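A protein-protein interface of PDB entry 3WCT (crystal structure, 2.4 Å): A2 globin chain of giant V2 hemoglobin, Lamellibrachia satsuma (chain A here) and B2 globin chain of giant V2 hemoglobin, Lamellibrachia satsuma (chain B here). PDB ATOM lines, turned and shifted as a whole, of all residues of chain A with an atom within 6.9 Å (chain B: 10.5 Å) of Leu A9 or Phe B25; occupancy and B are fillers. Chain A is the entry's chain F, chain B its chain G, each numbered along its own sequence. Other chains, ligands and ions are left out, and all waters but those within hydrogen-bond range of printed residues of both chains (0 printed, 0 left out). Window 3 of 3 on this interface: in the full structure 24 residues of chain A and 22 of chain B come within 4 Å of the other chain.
The backbone carbonyl oxygen (O) of Ser B22 lies within hydrogen-bond range of the guanidinium group (NE) of Arg B29 (2.9 Å).
NZ of Lys A12 sits at hydrogen-bond distance from O of Ala A76.
The side-chain amino group (NZ) of Lys A12 sits at hydrogen-bond distance from the backbone carbonyl oxygen (O) of Val A75 (3.1 Å).
The side-chain amino group (NZ) of Lys A12 lies within salt-bridge range of the side-chain carboxylate (OD2) of Asp A79, 2.8 Å away.
The side-chain hydroxyl of Ser B22 sits at hydrogen-bond distance from the backbone carbonyl oxygen of Phe B25, 2.8 Å away.
The backbone carbonyl oxygen of Phe B25 is in hydrogen-bond range of the guanidinium group of Arg B29, at 3.2 Å.
Among the printed residues, merely in contact across the chains: Leu A9 with Phe B25, Lys A12 with Phe B25, Arg A13 with Gln B24, Ala A76 with Gln B24, Ala A76 with Phe B25, Ala A76 with Thr B26, Ala A76 with Arg B29, Leu A77 with Thr B26, Leu A77 with Ile B69 and Asp A79 with Phe B25.
Printed residues of chain A that touch a printed residue of chain B: Leu A9, Lys A12, Arg A13, Ala A76, Leu A77 and Asp A79.
Of the 19 printed residues of chain B, 5 touch a printed residue of chain A.
Along chain B the printed residues that touch a printed residue of chain A span positions 24 to 69.
Among the printed residues, no Asp or Glu carboxylate lies within 4 Å of a Lys or Arg side-chain nitrogen of the other chain.
The side-chain amino group (NZ) of Lys A12 lies within hydrogen-bond range of the backbone carbonyl oxygen (O) of Gln B24, at 2.8 Å.
Leu A9 touches one residue of chain B.
Phe B25 touches just these residues of chain A: Leu A9 (3.6 Å), Lys A12 (3.4 Å), Ala A76 (3.8 Å) and Asp A79 (3.5 Å).
Of chain B, only Gln B24 (2.8 Å) and Phe B25 (3.4 Å) come within 4 Å of Lys A12.
Ala A76 touches four residues of chain B.
Of the printed residues of chain B, Leu A77 touches Thr B26 and Ile B69.
Of the printed residues of chain A, Thr B26 touches Ala A76 and Leu A77.
Leu B30 touches none of the printed residues of chain A.
The nearest residue of chain B that does not touch Leu A9 is Gln B24 (4.5 Å).
The nearest residue of chain A that does not touch Phe B25 is Leu A77 (6.0 Å).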
ATOM      1  N   GLY A   4      -6.375  16.806  -9.339  1.00  0.00           N
ATOM      2  CA  GLY A   4      -7.465  16.083  -9.970  1.00  0.00           C
ATOM      3  C   GLY A   4      -8.789  16.795  -9.752  1.00  0.00           C
ATOM      4  O   GLY A   4      -8.800  17.908  -9.242  1.00  0.00           O
ATOM      5  N   PRO A   5      -9.925  16.180 -10.123  1.00  0.00           N
ATOM      6  CA  PRO A   5     -11.252  16.792  -9.953  1.00  0.00           C
ATOM      7  C   PRO A   5     -11.617  17.094  -8.499  1.00  0.00           C
ATOM      8  O   PRO A   5     -12.204  18.134  -8.211  1.00  0.00           O
ATOM      9  CB  PRO A   5     -12.194  15.758 -10.564  1.00  0.00           C
ATOM     10  CG  PRO A   5     -11.332  15.089 -11.610  1.00  0.00           C
ATOM     11  CD  PRO A   5     -10.023  14.924 -10.889  1.00  0.00           C
ATOM     12  N   LEU A   6     -11.260  16.184  -7.594  1.00  0.00           N
ATOM     13  CA  LEU A   6     -11.560  16.341  -6.166  1.00  0.00           C
ATOM     14  C   LEU A   6     -10.721  17.424  -5.500  1.00  0.00           C
ATOM     15  O   LEU A   6     -11.223  18.175  -4.672  1.00  0.00           O
ATOM     16  CB  LEU A   6     -11.358  15.012  -5.430  1.00  0.00           C
ATOM     17  CG  LEU A   6     -12.149  13.816  -5.962  1.00  0.00           C
ATOM     18  CD1 LEU A   6     -11.833  12.587  -5.118  1.00  0.00           C
ATOM     19  CD2 LEU A   6     -13.642  14.106  -5.935  1.00  0.00           C
ATOM     20  N   GLN A   7      -9.440  17.504  -5.842  1.00  0.00           N
ATOM     21  CA  GLN A   7      -8.588  18.537  -5.263  1.00  0.00           C
ATOM     22  C   GLN A   7      -9.054  19.918  -5.732  1.00  0.00           C
ATOM     23  O   GLN A   7      -8.903  20.915  -5.023  1.00  0.00           O
ATOM     24  CB  GLN A   7      -7.134  18.335  -5.680  1.00  0.00           C
ATOM     25  CG  GLN A   7      -6.454  17.121  -5.075  1.00  0.00           C
ATOM     26  CD  GLN A   7      -6.973  15.812  -5.631  1.00  0.00           C
ATOM     27  OE1 GLN A   7      -7.252  15.696  -6.829  1.00  0.00           O
ATOM     28  NE2 GLN A   7      -7.080  14.805  -4.766  1.00  0.00           N
ATOM     29  N   ARG A   8      -9.627  19.978  -6.932  1.00  0.00           N
ATOM     30  CA  ARG A   8     -10.106  21.249  -7.472  1.00  0.00           C
ATOM     31  C   ARG A   8     -11.372  21.710  -6.768  1.00  0.00           C
ATOM     32  O   ARG A   8     -11.584  22.914  -6.603  1.00  0.00           O
ATOM     33  CB  ARG A   8     -10.349  21.127  -8.982  1.00  0.00           C
ATOM     34  CG  ARG A   8      -9.070  20.864  -9.755  1.00  0.00           C
ATOM     35  CD  ARG A   8      -9.317  20.561 -11.218  1.00  0.00           C
ATOM     36  NE  ARG A   8      -8.054  20.194 -11.843  1.00  0.00           N
ATOM     37  CZ  ARG A   8      -7.452  20.887 -12.801  1.00  0.00           C
ATOM     38  NH1 ARG A   8      -8.001  21.998 -13.276  1.00  0.00           N
ATOM     39  NH2 ARG A   8      -6.276  20.479 -13.259  1.00  0.00           N
ATOM     40  N   LEU A   9     -12.213  20.757  -6.370  1.00  0.00           N
ATOM     41  CA  LEU A   9     -13.436  21.099  -5.657  1.00  0.00           C
ATOM     42  C   LEU A   9     -13.076  21.592  -4.254  1.00  0.00           C
ATOM     43  O   LEU A   9     -13.665  22.534  -3.759  1.00  0.00           O
ATOM     44  CB  LEU A   9     -14.373  19.894  -5.544  1.00  0.00           C
ATOM     45  CG  LEU A   9     -15.181  19.497  -6.785  1.00  0.00           C
ATOM     46  CD1 LEU A   9     -16.124  18.341  -6.418  1.00  0.00           C
ATOM     47  CD2 LEU A   9     -15.992  20.684  -7.305  1.00  0.00           C
ATOM     48  N   LYS A  10     -12.103  20.936  -3.632  1.00  0.00           N
ATOM     49  CA  LYS A  10     -11.628  21.281  -2.294  1.00  0.00           C
ATOM     50  C   LYS A  10     -11.059  22.701  -2.307  1.00  0.00           C
ATOM     51  O   LYS A  10     -11.444  23.562  -1.507  1.00  0.00           O
ATOM     52  CB  LYS A  10     -10.511  20.316  -1.880  1.00  0.00           C
ATOM     53  CG  LYS A  10     -10.156  20.308  -0.403  1.00  0.00           C
ATOM     54  CD  LYS A  10     -11.223  19.562   0.390  1.00  0.00           C
ATOM     55  CE  LYS A  10     -10.833  19.373   1.852  1.00  0.00           C
ATOM     56  NZ  LYS A  10      -9.781  18.332   2.062  1.00  0.00           N
ATOM     57  N   VAL A  11     -10.128  22.919  -3.227  1.00  0.00           N
ATOM     58  CA  VAL A  11      -9.468  24.203  -3.376  1.00  0.00           C
ATOM     59  C   VAL A  11     -10.479  25.297  -3.629  1.00  0.00           C
ATOM     60  O   VAL A  11     -10.314  26.410  -3.126  1.00  0.00           O
ATOM     61  CB  VAL A  11      -8.427  24.172  -4.521  1.00  0.00           C
ATOM     62  CG1 VAL A  11      -7.928  25.577  -4.840  1.00  0.00           C
ATOM     63  CG2 VAL A  11      -7.261  23.287  -4.115  1.00  0.00           C
ATOM     64  N   LYS A  12     -11.528  24.986  -4.391  1.00  0.00           N
ATOM     65  CA  LYS A  12     -12.573  25.972  -4.670  1.00  0.00           C
ATOM     66  C   LYS A  12     -13.268  26.383  -3.385  1.00  0.00           C
ATOM     67  O   LYS A  12     -13.444  27.573  -3.109  1.00  0.00           O
ATOM     68  CB  LYS A  12     -13.642  25.406  -5.613  1.00  0.00           C
ATOM     69  CG  LYS A  12     -13.277  25.380  -7.076  1.00  0.00           C
ATOM     70  CD  LYS A  12     -14.402  24.718  -7.872  1.00  0.00           C
ATOM     71  CE  LYS A  12     -14.147  24.774  -9.368  1.00  0.00           C
ATOM     72  NZ  LYS A  12     -14.303  26.150  -9.932  1.00  0.00           N
ATOM     73  N   ARG A  13     -13.685  25.379  -2.614  1.00  0.00           N
ATOM     74  CA  ARG A  13     -14.386  25.640  -1.372  1.00  0.00           C
ATOM     75  C   ARG A  13     -13.512  26.373  -0.354  1.00  0.00           C
ATOM     76  O   ARG A  13     -13.905  27.420   0.140  1.00  0.00           O
ATOM     77  CB  ARG A  13     -14.926  24.334  -0.760  1.00  0.00           C
ATOM     78  CG  ARG A  13     -15.926  24.566   0.383  1.00  0.00           C
ATOM     79  CD  ARG A  13     -16.668  23.287   0.752  1.00  0.00           C
ATOM     80  NE  ARG A  13     -15.752  22.176   1.009  1.00  0.00           N
ATOM     81  CZ  ARG A  13     -14.965  22.090   2.072  1.00  0.00           C
ATOM     82  NH1 ARG A  13     -14.159  21.037   2.209  1.00  0.00           N
ATOM     83  NH2 ARG A  13     -14.995  23.047   3.007  1.00  0.00           N
ATOM     84  N   GLN A  14     -12.333  25.847  -0.051  1.00  0.00           N
ATOM     85  CA  GLN A  14     -11.496  26.504   0.937  1.00  0.00           C
ATOM     86  C   GLN A  14     -11.160  27.909   0.460  1.00  0.00           C
ATOM     87  O   GLN A  14     -11.186  28.855   1.245  1.00  0.00           O
ATOM     88  CB  GLN A  14     -10.236  25.671   1.233  1.00  0.00           C
ATOM     89  CG  GLN A  14     -10.566  24.258   1.700  1.00  0.00           C
ATOM     90  CD  GLN A  14      -9.424  23.578   2.456  1.00  0.00           C
ATOM     91  OE1 GLN A  14      -8.248  23.781   2.150  1.00  0.00           O
ATOM     92  NE2 GLN A  14      -9.778  22.744   3.445  1.00  0.00           N
ATOM     93  N   TRP A  15     -10.885  28.062  -0.831  1.00  0.00           N
ATOM     94  CA  TRP A  15     -10.588  29.394  -1.355  1.00  0.00           C
ATOM     95  C   TRP A  15     -11.752  30.357  -1.083  1.00  0.00           C
ATOM     96  O   TRP A  15     -11.542  31.505  -0.670  1.00  0.00           O
ATOM     97  CB  TRP A  15     -10.301  29.347  -2.860  1.00  0.00           C
ATOM     98  CG  TRP A  15     -10.294  30.707  -3.476  1.00  0.00           C
ATOM     99  CD1 TRP A  15     -11.303  31.280  -4.182  1.00  0.00           C
ATOM    100  CD2 TRP A  15      -9.270  31.703  -3.350  1.00  0.00           C
ATOM    101  NE1 TRP A  15     -10.977  32.578  -4.503  1.00  0.00           N
ATOM    102  CE2 TRP A  15      -9.735  32.863  -4.006  1.00  0.00           C
ATOM    103  CE3 TRP A  15      -8.007  31.728  -2.745  1.00  0.00           C
ATOM    104  CZ2 TRP A  15      -8.983  34.046  -4.077  1.00  0.00           C
ATOM    105  CZ3 TRP A  15      -7.254  32.911  -2.811  1.00  0.00           C
ATOM    106  CH2 TRP A  15      -7.749  34.052  -3.475  1.00  0.00           C
ATOM    107  N   VAL A  75      -9.091  29.938  -9.732  1.00  0.00           N
ATOM    108  CA  VAL A  75      -9.713  28.970  -8.853  1.00  0.00           C
ATOM    109  C   VAL A  75     -11.129  28.722  -9.364  1.00  0.00           C
ATOM    110  O   VAL A  75     -11.549  27.575  -9.486  1.00  0.00           O
ATOM    111  CB  VAL A  75      -9.721  29.491  -7.379  1.00  0.00           C
ATOM    112  CG1 VAL A  75     -10.801  28.808  -6.566  1.00  0.00           C
ATOM    113  CG2 VAL A  75      -8.360  29.233  -6.750  1.00  0.00           C
ATOM    114  N   ALA A  76     -11.844  29.804  -9.676  1.00  0.00           N
ATOM    115  CA  ALA A  76     -13.210  29.703 -10.179  1.00  0.00           C
ATOM    116  C   ALA A  76     -13.281  28.881 -11.480  1.00  0.00           C
ATOM    117  O   ALA A  76     -14.312  28.279 -11.777  1.00  0.00           O
ATOM    118  CB  ALA A  76     -13.796  31.108 -10.410  1.00  0.00           C
ATOM    119  N   LEU A  77     -12.176  28.844 -12.227  1.00  0.00           N
ATOM    120  CA  LEU A  77     -12.105  28.126 -13.501  1.00  0.00           C
ATOM    121  C   LEU A  77     -11.340  26.806 -13.480  1.00  0.00           C
ATOM    122  O   LEU A  77     -11.008  26.273 -14.539  1.00  0.00           O
ATOM    123  CB  LEU A  77     -11.467  29.035 -14.557  1.00  0.00           C
ATOM    124  CG  LEU A  77     -12.316  30.244 -14.957  1.00  0.00           C
ATOM    125  CD1 LEU A  77     -11.477  31.297 -15.668  1.00  0.00           C
ATOM    126  CD2 LEU A  77     -13.445  29.758 -15.820  1.00  0.00           C
ATOM    127  N   LEU A  78     -11.050  26.270 -12.300  1.00  0.00           N
ATOM    128  CA  LEU A  78     -10.299  25.019 -12.230  1.00  0.00           C
ATOM    129  C   LEU A  78     -11.068  23.859 -12.838  1.00  0.00           C
ATOM    130  O   LEU A  78     -10.485  22.827 -13.167  1.00  0.00           O
ATOM    131  CB  LEU A  78      -9.926  24.692 -10.781  1.00  0.00           C
ATOM    132  CG  LEU A  78      -8.781  25.528 -10.186  1.00  0.00           C
ATOM    133  CD1 LEU A  78      -8.611  25.196  -8.714  1.00  0.00           C
ATOM    134  CD2 LEU A  78      -7.482  25.251 -10.955  1.00  0.00           C
ATOM    135  N   ASP A  79     -12.372  24.058 -13.003  1.00  0.00           N
ATOM    136  CA  ASP A  79     -13.272  23.044 -13.539  1.00  0.00           C
ATOM    137  C   ASP A  79     -13.571  23.211 -15.030  1.00  0.00           C
ATOM    138  O   ASP A  79     -14.232  22.365 -15.618  1.00  0.00           O
ATOM    139  CB  ASP A  79     -14.593  23.103 -12.783  1.00  0.00           C
ATOM    140  CG  ASP A  79     -15.349  24.383 -13.070  1.00  0.00           C
ATOM    141  OD1 ASP A  79     -16.321  24.347 -13.852  1.00  0.00           O
ATOM    142  OD2 ASP A  79     -14.950  25.437 -12.531  1.00  0.00           O
ATOM    143  N   CYS A 133      -2.821  22.096  -7.126  1.00  0.00           N
ATOM    144  CA  CYS A 133      -3.530  23.024  -7.999  1.00  0.00           C
ATOM    145  C   CYS A 133      -2.842  24.395  -8.173  1.00  0.00           C
ATOM    146  O   CYS A 133      -3.029  25.065  -9.202  1.00  0.00           O
ATOM    147  CB  CYS A 133      -4.978  23.176  -7.530  1.00  0.00           C
ATOM    148  SG  CYS A 133      -5.961  21.629  -7.624  1.00  0.00           S
ATOM    149  N   ALA B  18     -23.576  40.252  -3.773  1.00  0.00           N
ATOM    150  CA  ALA B  18     -23.247  39.038  -3.035  1.00  0.00           C
ATOM    151  C   ALA B  18     -24.120  37.887  -3.478  1.00  0.00           C
ATOM    152  O   ALA B  18     -23.696  37.033  -4.254  1.00  0.00           O
ATOM    153  CB  ALA B  18     -23.417  39.271  -1.542  1.00  0.00           C
ATOM    154  N   ASN B  19     -25.345  37.872  -2.971  1.00  0.00           N
ATOM    155  CA  ASN B  19     -26.322  36.840  -3.297  1.00  0.00           C
ATOM    156  C   ASN B  19     -26.061  36.217  -4.668  1.00  0.00           C
ATOM    157  O   ASN B  19     -25.827  35.010  -4.784  1.00  0.00           O
ATOM    158  CB  ASN B  19     -27.739  37.442  -3.283  1.00  0.00           C
ATOM    159  CG  ASN B  19     -28.329  37.553  -1.880  1.00  0.00           C
ATOM    160  OD1 ASN B  19     -27.620  37.812  -0.905  1.00  0.00           O
ATOM    161  ND2 ASN B  19     -29.644  37.377  -1.780  1.00  0.00           N
ATOM    162  N   VAL B  20     -26.076  37.059  -5.697  1.00  0.00           N
ATOM    163  CA  VAL B  20     -25.898  36.613  -7.071  1.00  0.00           C
ATOM    164  C   VAL B  20     -24.519  36.130  -7.527  1.00  0.00           C
ATOM    165  O   VAL B  20     -24.422  35.405  -8.513  1.00  0.00           O
ATOM    166  CB  VAL B  20     -26.364  37.713  -8.014  1.00  0.00           C
ATOM    167  CG1 VAL B  20     -26.211  37.274  -9.440  1.00  0.00           C
ATOM    168  CG2 VAL B  20     -27.810  38.048  -7.709  1.00  0.00           C
ATOM    169  N   TRP B  21     -23.464  36.506  -6.811  1.00  0.00           N
ATOM    170  CA  TRP B  21     -22.098  36.126  -7.184  1.00  0.00           C
ATOM    171  C   TRP B  21     -21.569  34.844  -6.529  1.00  0.00           C
ATOM    172  O   TRP B  21     -21.309  34.813  -5.324  1.00  0.00           O
ATOM    173  CB  TRP B  21     -21.171  37.319  -6.899  1.00  0.00           C
ATOM    174  CG  TRP B  21     -19.721  37.013  -6.671  1.00  0.00           C
ATOM    175  CD1 TRP B  21     -19.148  36.556  -5.516  1.00  0.00           C
ATOM    176  CD2 TRP B  21     -18.651  37.209  -7.596  1.00  0.00           C
ATOM    177  NE1 TRP B  21     -17.788  36.463  -5.665  1.00  0.00           N
ATOM    178  CE2 TRP B  21     -17.454  36.860  -6.932  1.00  0.00           C
ATOM    179  CE3 TRP B  21     -18.584  37.652  -8.919  1.00  0.00           C
ATOM    180  CZ2 TRP B  21     -16.204  36.936  -7.549  1.00  0.00           C
ATOM    181  CZ3 TRP B  21     -17.340  37.728  -9.536  1.00  0.00           C
ATOM    182  CH2 TRP B  21     -16.166  37.373  -8.847  1.00  0.00           C
ATOM    183  N   SER B  22     -21.415  33.782  -7.322  1.00  0.00           N
ATOM    184  CA  SER B  22     -20.909  32.510  -6.795  1.00  0.00           C
ATOM    185  C   SER B  22     -19.388  32.576  -6.638  1.00  0.00           C
ATOM    186  O   SER B  22     -18.653  32.794  -7.607  1.00  0.00           O
ATOM    187  CB  SER B  22     -21.300  31.334  -7.709  1.00  0.00           C
ATOM    188  OG  SER B  22     -20.688  31.422  -8.983  1.00  0.00           O
ATOM    189  N   ALA B  23     -18.925  32.385  -5.406  1.00  0.00           N
ATOM    190  CA  ALA B  23     -17.505  32.454  -5.086  1.00  0.00           C
ATOM    191  C   ALA B  23     -16.697  31.193  -5.400  1.00  0.00           C
ATOM    192  O   ALA B  23     -15.484  31.169  -5.184  1.00  0.00           O
ATOM    193  CB  ALA B  23     -17.339  32.823  -3.613  1.00  0.00           C
ATOM    194  N   GLN B  24     -17.357  30.160  -5.918  1.00  0.00           N
ATOM    195  CA  GLN B  24     -16.675  28.904  -6.236  1.00  0.00           C
ATOM    196  C   GLN B  24     -16.611  28.511  -7.714  1.00  0.00           C
ATOM    197  O   GLN B  24     -15.658  27.857  -8.140  1.00  0.00           O
ATOM    198  CB  GLN B  24     -17.305  27.755  -5.447  1.00  0.00           C
ATOM    199  CG  GLN B  24     -16.826  27.656  -4.018  1.00  0.00           C
ATOM    200  CD  GLN B  24     -17.300  26.385  -3.333  1.00  0.00           C
ATOM    201  OE1 GLN B  24     -17.223  25.292  -3.896  1.00  0.00           O
ATOM    202  NE2 GLN B  24     -17.778  26.522  -2.107  1.00  0.00           N
ATOM    203  N   PHE B  25     -17.625  28.890  -8.488  1.00  0.00           N
ATOM    204  CA  PHE B  25     -17.662  28.551  -9.907  1.00  0.00           C
ATOM    205  C   PHE B  25     -17.923  29.789 -10.748  1.00  0.00           C
ATOM    206  O   PHE B  25     -18.185  30.862 -10.214  1.00  0.00           O
ATOM    207  CB  PHE B  25     -18.739  27.499 -10.162  1.00  0.00           C
ATOM    208  CG  PHE B  25     -18.402  26.144  -9.600  1.00  0.00           C
ATOM    209  CD1 PHE B  25     -17.731  25.201 -10.375  1.00  0.00           C
ATOM    210  CD2 PHE B  25     -18.734  25.818  -8.280  1.00  0.00           C
ATOM    211  CE1 PHE B  25     -17.398  23.953  -9.849  1.00  0.00           C
ATOM    212  CE2 PHE B  25     -18.405  24.572  -7.741  1.00  0.00           C
ATOM    213  CZ  PHE B  25     -17.735  23.639  -8.527  1.00  0.00           C
ATOM    214  N   THR B  26     -17.857  29.643 -12.065  1.00  0.00           N
ATOM    215  CA  THR B  26     -18.070  30.781 -12.952  1.00  0.00           C
ATOM    216  C   THR B  26     -19.366  30.765 -13.756  1.00  0.00           C
ATOM    217  O   THR B  26     -19.693  31.749 -14.421  1.00  0.00           O
ATOM    218  CB  THR B  26     -16.897  30.926 -13.933  1.00  0.00           C
ATOM    219  OG1 THR B  26     -16.672  29.677 -14.604  1.00  0.00           O
ATOM    220  CG2 THR B  26     -15.638  31.338 -13.188  1.00  0.00           C
ATOM    221  N   GLY B  27     -20.102  29.660 -13.695  1.00  0.00           N
ATOM    222  CA  GLY B  27     -21.343  29.580 -14.442  1.00  0.00           C
ATOM    223  C   GLY B  27     -22.212  30.813 -14.275  1.00  0.00           C
ATOM    224  O   GLY B  27     -22.574  31.478 -15.245  1.00  0.00           O
ATOM    225  N   ARG B  28     -22.540  31.134 -13.033  1.00  0.00           N
ATOM    226  CA  ARG B  28     -23.384  32.284 -12.775  1.00  0.00           C
ATOM    227  C   ARG B  28     -22.711  33.605 -13.159  1.00  0.00           C
ATOM    228  O   ARG B  28     -23.375  34.512 -13.657  1.00  0.00           O
ATOM    229  CB  ARG B  28     -23.825  32.288 -11.304  1.00  0.00           C
ATOM    230  CG  ARG B  28     -24.819  33.376 -10.952  1.00  0.00           C
ATOM    231  CD  ARG B  28     -25.773  32.947  -9.836  1.00  0.00           C
ATOM    232  NE  ARG B  28     -25.078  32.541  -8.619  1.00  0.00           N
ATOM    233  CZ  ARG B  28     -25.005  31.286  -8.180  1.00  0.00           C
ATOM    234  NH1 ARG B  28     -24.351  31.004  -7.057  1.00  0.00           N
ATOM    235  NH2 ARG B  28     -25.592  30.306  -8.860  1.00  0.00           N
ATOM    236  N   ARG B  29     -21.403  33.712 -12.951  1.00  0.00           N
ATOM    237  CA  ARG B  29     -20.689  34.944 -13.293  1.00  0.00           C
ATOM    238  C   ARG B  29     -20.737  35.181 -14.802  1.00  0.00           C
ATOM    239  O   ARG B  29     -20.977  36.300 -15.280  1.00  0.00           O
ATOM    240  CB  ARG B  29     -19.219  34.854 -12.879  1.00  0.00           C
ATOM    241  CG  ARG B  29     -18.968  34.425 -11.446  1.00  0.00           C
ATOM    242  CD  ARG B  29     -17.461  34.363 -11.180  1.00  0.00           C
ATOM    243  NE  ARG B  29     -17.148  33.881  -9.839  1.00  0.00           N
ATOM    244  CZ  ARG B  29     -15.945  33.960  -9.280  1.00  0.00           C
ATOM    245  NH1 ARG B  29     -14.933  34.506  -9.947  1.00  0.00           N
ATOM    246  NH2 ARG B  29     -15.755  33.503  -8.052  1.00  0.00           N
ATOM    247  N   LEU B  30     -20.497  34.101 -15.534  1.00  0.00           N
ATOM    248  CA  LEU B  30     -20.461  34.089 -16.989  1.00  0.00           C
ATOM    249  C   LEU B  30     -21.801  34.486 -17.608  1.00  0.00           C
ATOM    250  O   LEU B  30     -21.885  35.411 -18.411  1.00  0.00           O
ATOM    251  CB  LEU B  30     -20.073  32.684 -17.437  1.00  0.00           C
ATOM    252  CG  LEU B  30     -19.254  32.529 -18.702  1.00  0.00           C
ATOM    253  CD1 LEU B  30     -18.108  33.545 -18.699  1.00  0.00           C
ATOM    254  CD2 LEU B  30     -18.735  31.092 -18.774  1.00  0.00           C
ATOM    255  N   ALA B  31     -22.845  33.772 -17.218  1.00  0.00           N
ATOM    256  CA  ALA B  31     -24.181  34.034 -17.715  1.00  0.00           C
ATOM    257  C   ALA B  31     -24.586  35.507 -17.564  1.00  0.00           C
ATOM    258  O   ALA B  31     -25.246  36.069 -18.442  1.00  0.00           O
ATOM    259  CB  ALA B  31     -25.161  33.150 -16.983  1.00  0.00           C
ATOM    260  N   ILE B  32     -24.194  36.126 -16.452  1.00  0.00           N
ATOM    261  CA  ILE B  32     -24.526  37.524 -16.186  1.00  0.00           C
ATOM    262  C   ILE B  32     -23.748  38.466 -17.095  1.00  0.00           C
ATOM    263  O   ILE B  32     -24.318  39.381 -17.696  1.00  0.00           O
ATOM    264  CB  ILE B  32     -24.210  37.905 -14.730  1.00  0.00           C
ATOM    265  CG1 ILE B  32     -25.032  37.036 -13.780  1.00  0.00           C
ATOM    266  CG2 ILE B  32     -24.499  39.396 -14.501  1.00  0.00           C
ATOM    267  CD1 ILE B  32     -24.720  37.264 -12.312  1.00  0.00           C
ATOM    268  N   ILE B  69     -15.294  36.948 -17.611  1.00  0.00           N
ATOM    269  CA  ILE B  69     -14.873  36.644 -16.267  1.00  0.00           C
ATOM    270  C   ILE B  69     -13.989  37.772 -15.734  1.00  0.00           C
ATOM    271  O   ILE B  69     -14.119  38.169 -14.576  1.00  0.00           O
ATOM    272  CB  ILE B  69     -14.142  35.282 -16.241  1.00  0.00           C
ATOM    273  CG1 ILE B  69     -15.181  34.174 -16.404  1.00  0.00           C
ATOM    274  CG2 ILE B  69     -13.347  35.112 -14.955  1.00  0.00           C
ATOM    275  CD1 ILE B  69     -14.601  32.775 -16.479  1.00  0.00           C
ATOM    276  N   VAL B  72     -16.360  40.890 -14.806  1.00  0.00           N
ATOM    277  CA  VAL B  72     -17.113  40.798 -13.566  1.00  0.00           C
ATOM    278  C   VAL B  72     -16.152  40.770 -12.373  1.00  0.00           C
ATOM    279  O   VAL B  72     -16.506  41.187 -11.286  1.00  0.00           O
ATOM    280  CB  VAL B  72     -18.064  39.566 -13.568  1.00  0.00           C
ATOM    281  CG1 VAL B  72     -19.274  39.860 -14.434  1.00  0.00           C
ATOM    282  CG2 VAL B  72     -17.362  38.358 -14.100  1.00  0.00           C
ATOM    283  N   ASN B  73     -14.932  40.287 -12.593  1.00  0.00           N
ATOM    284  CA  ASN B  73     -13.910  40.262 -11.549  1.00  0.00           C
ATOM    285  C   ASN B  73     -13.505  41.710 -11.252  1.00  0.00           C
ATOM    286  O   ASN B  73     -13.231  42.076 -10.106  1.00  0.00           O
ATOM    287  CB  ASN B  73     -12.681  39.481 -12.015  1.00  0.00           C
ATOM    288  CG  ASN B  73     -11.527  39.563 -11.024  1.00  0.00           C
ATOM    289  OD1 ASN B  73     -11.617  39.068  -9.897  1.00  0.00           O
ATOM    290  ND2 ASN B  73     -10.434  40.203 -11.441  1.00  0.00           N
ATOM    291  N   ASP B  76     -16.419  43.262  -9.505  1.00  0.00           N
ATOM    292  CA  ASP B  76     -16.478  42.674  -8.181  1.00  0.00           C
ATOM    293  C   ASP B  76     -15.500  43.352  -7.230  1.00  0.00           C
ATOM    294  O   ASP B  76     -15.848  43.672  -6.097  1.00  0.00           O
ATOM    295  CB  ASP B  76     -16.185  41.175  -8.251  1.00  0.00           C
ATOM    296  CG  ASP B  76     -16.137  40.536  -6.885  1.00  0.00           C
ATOM    297  OD1 ASP B  76     -15.022  40.331  -6.369  1.00  0.00           O
ATOM    298  OD2 ASP B  76     -17.214  40.259  -6.324  1.00  0.00           O
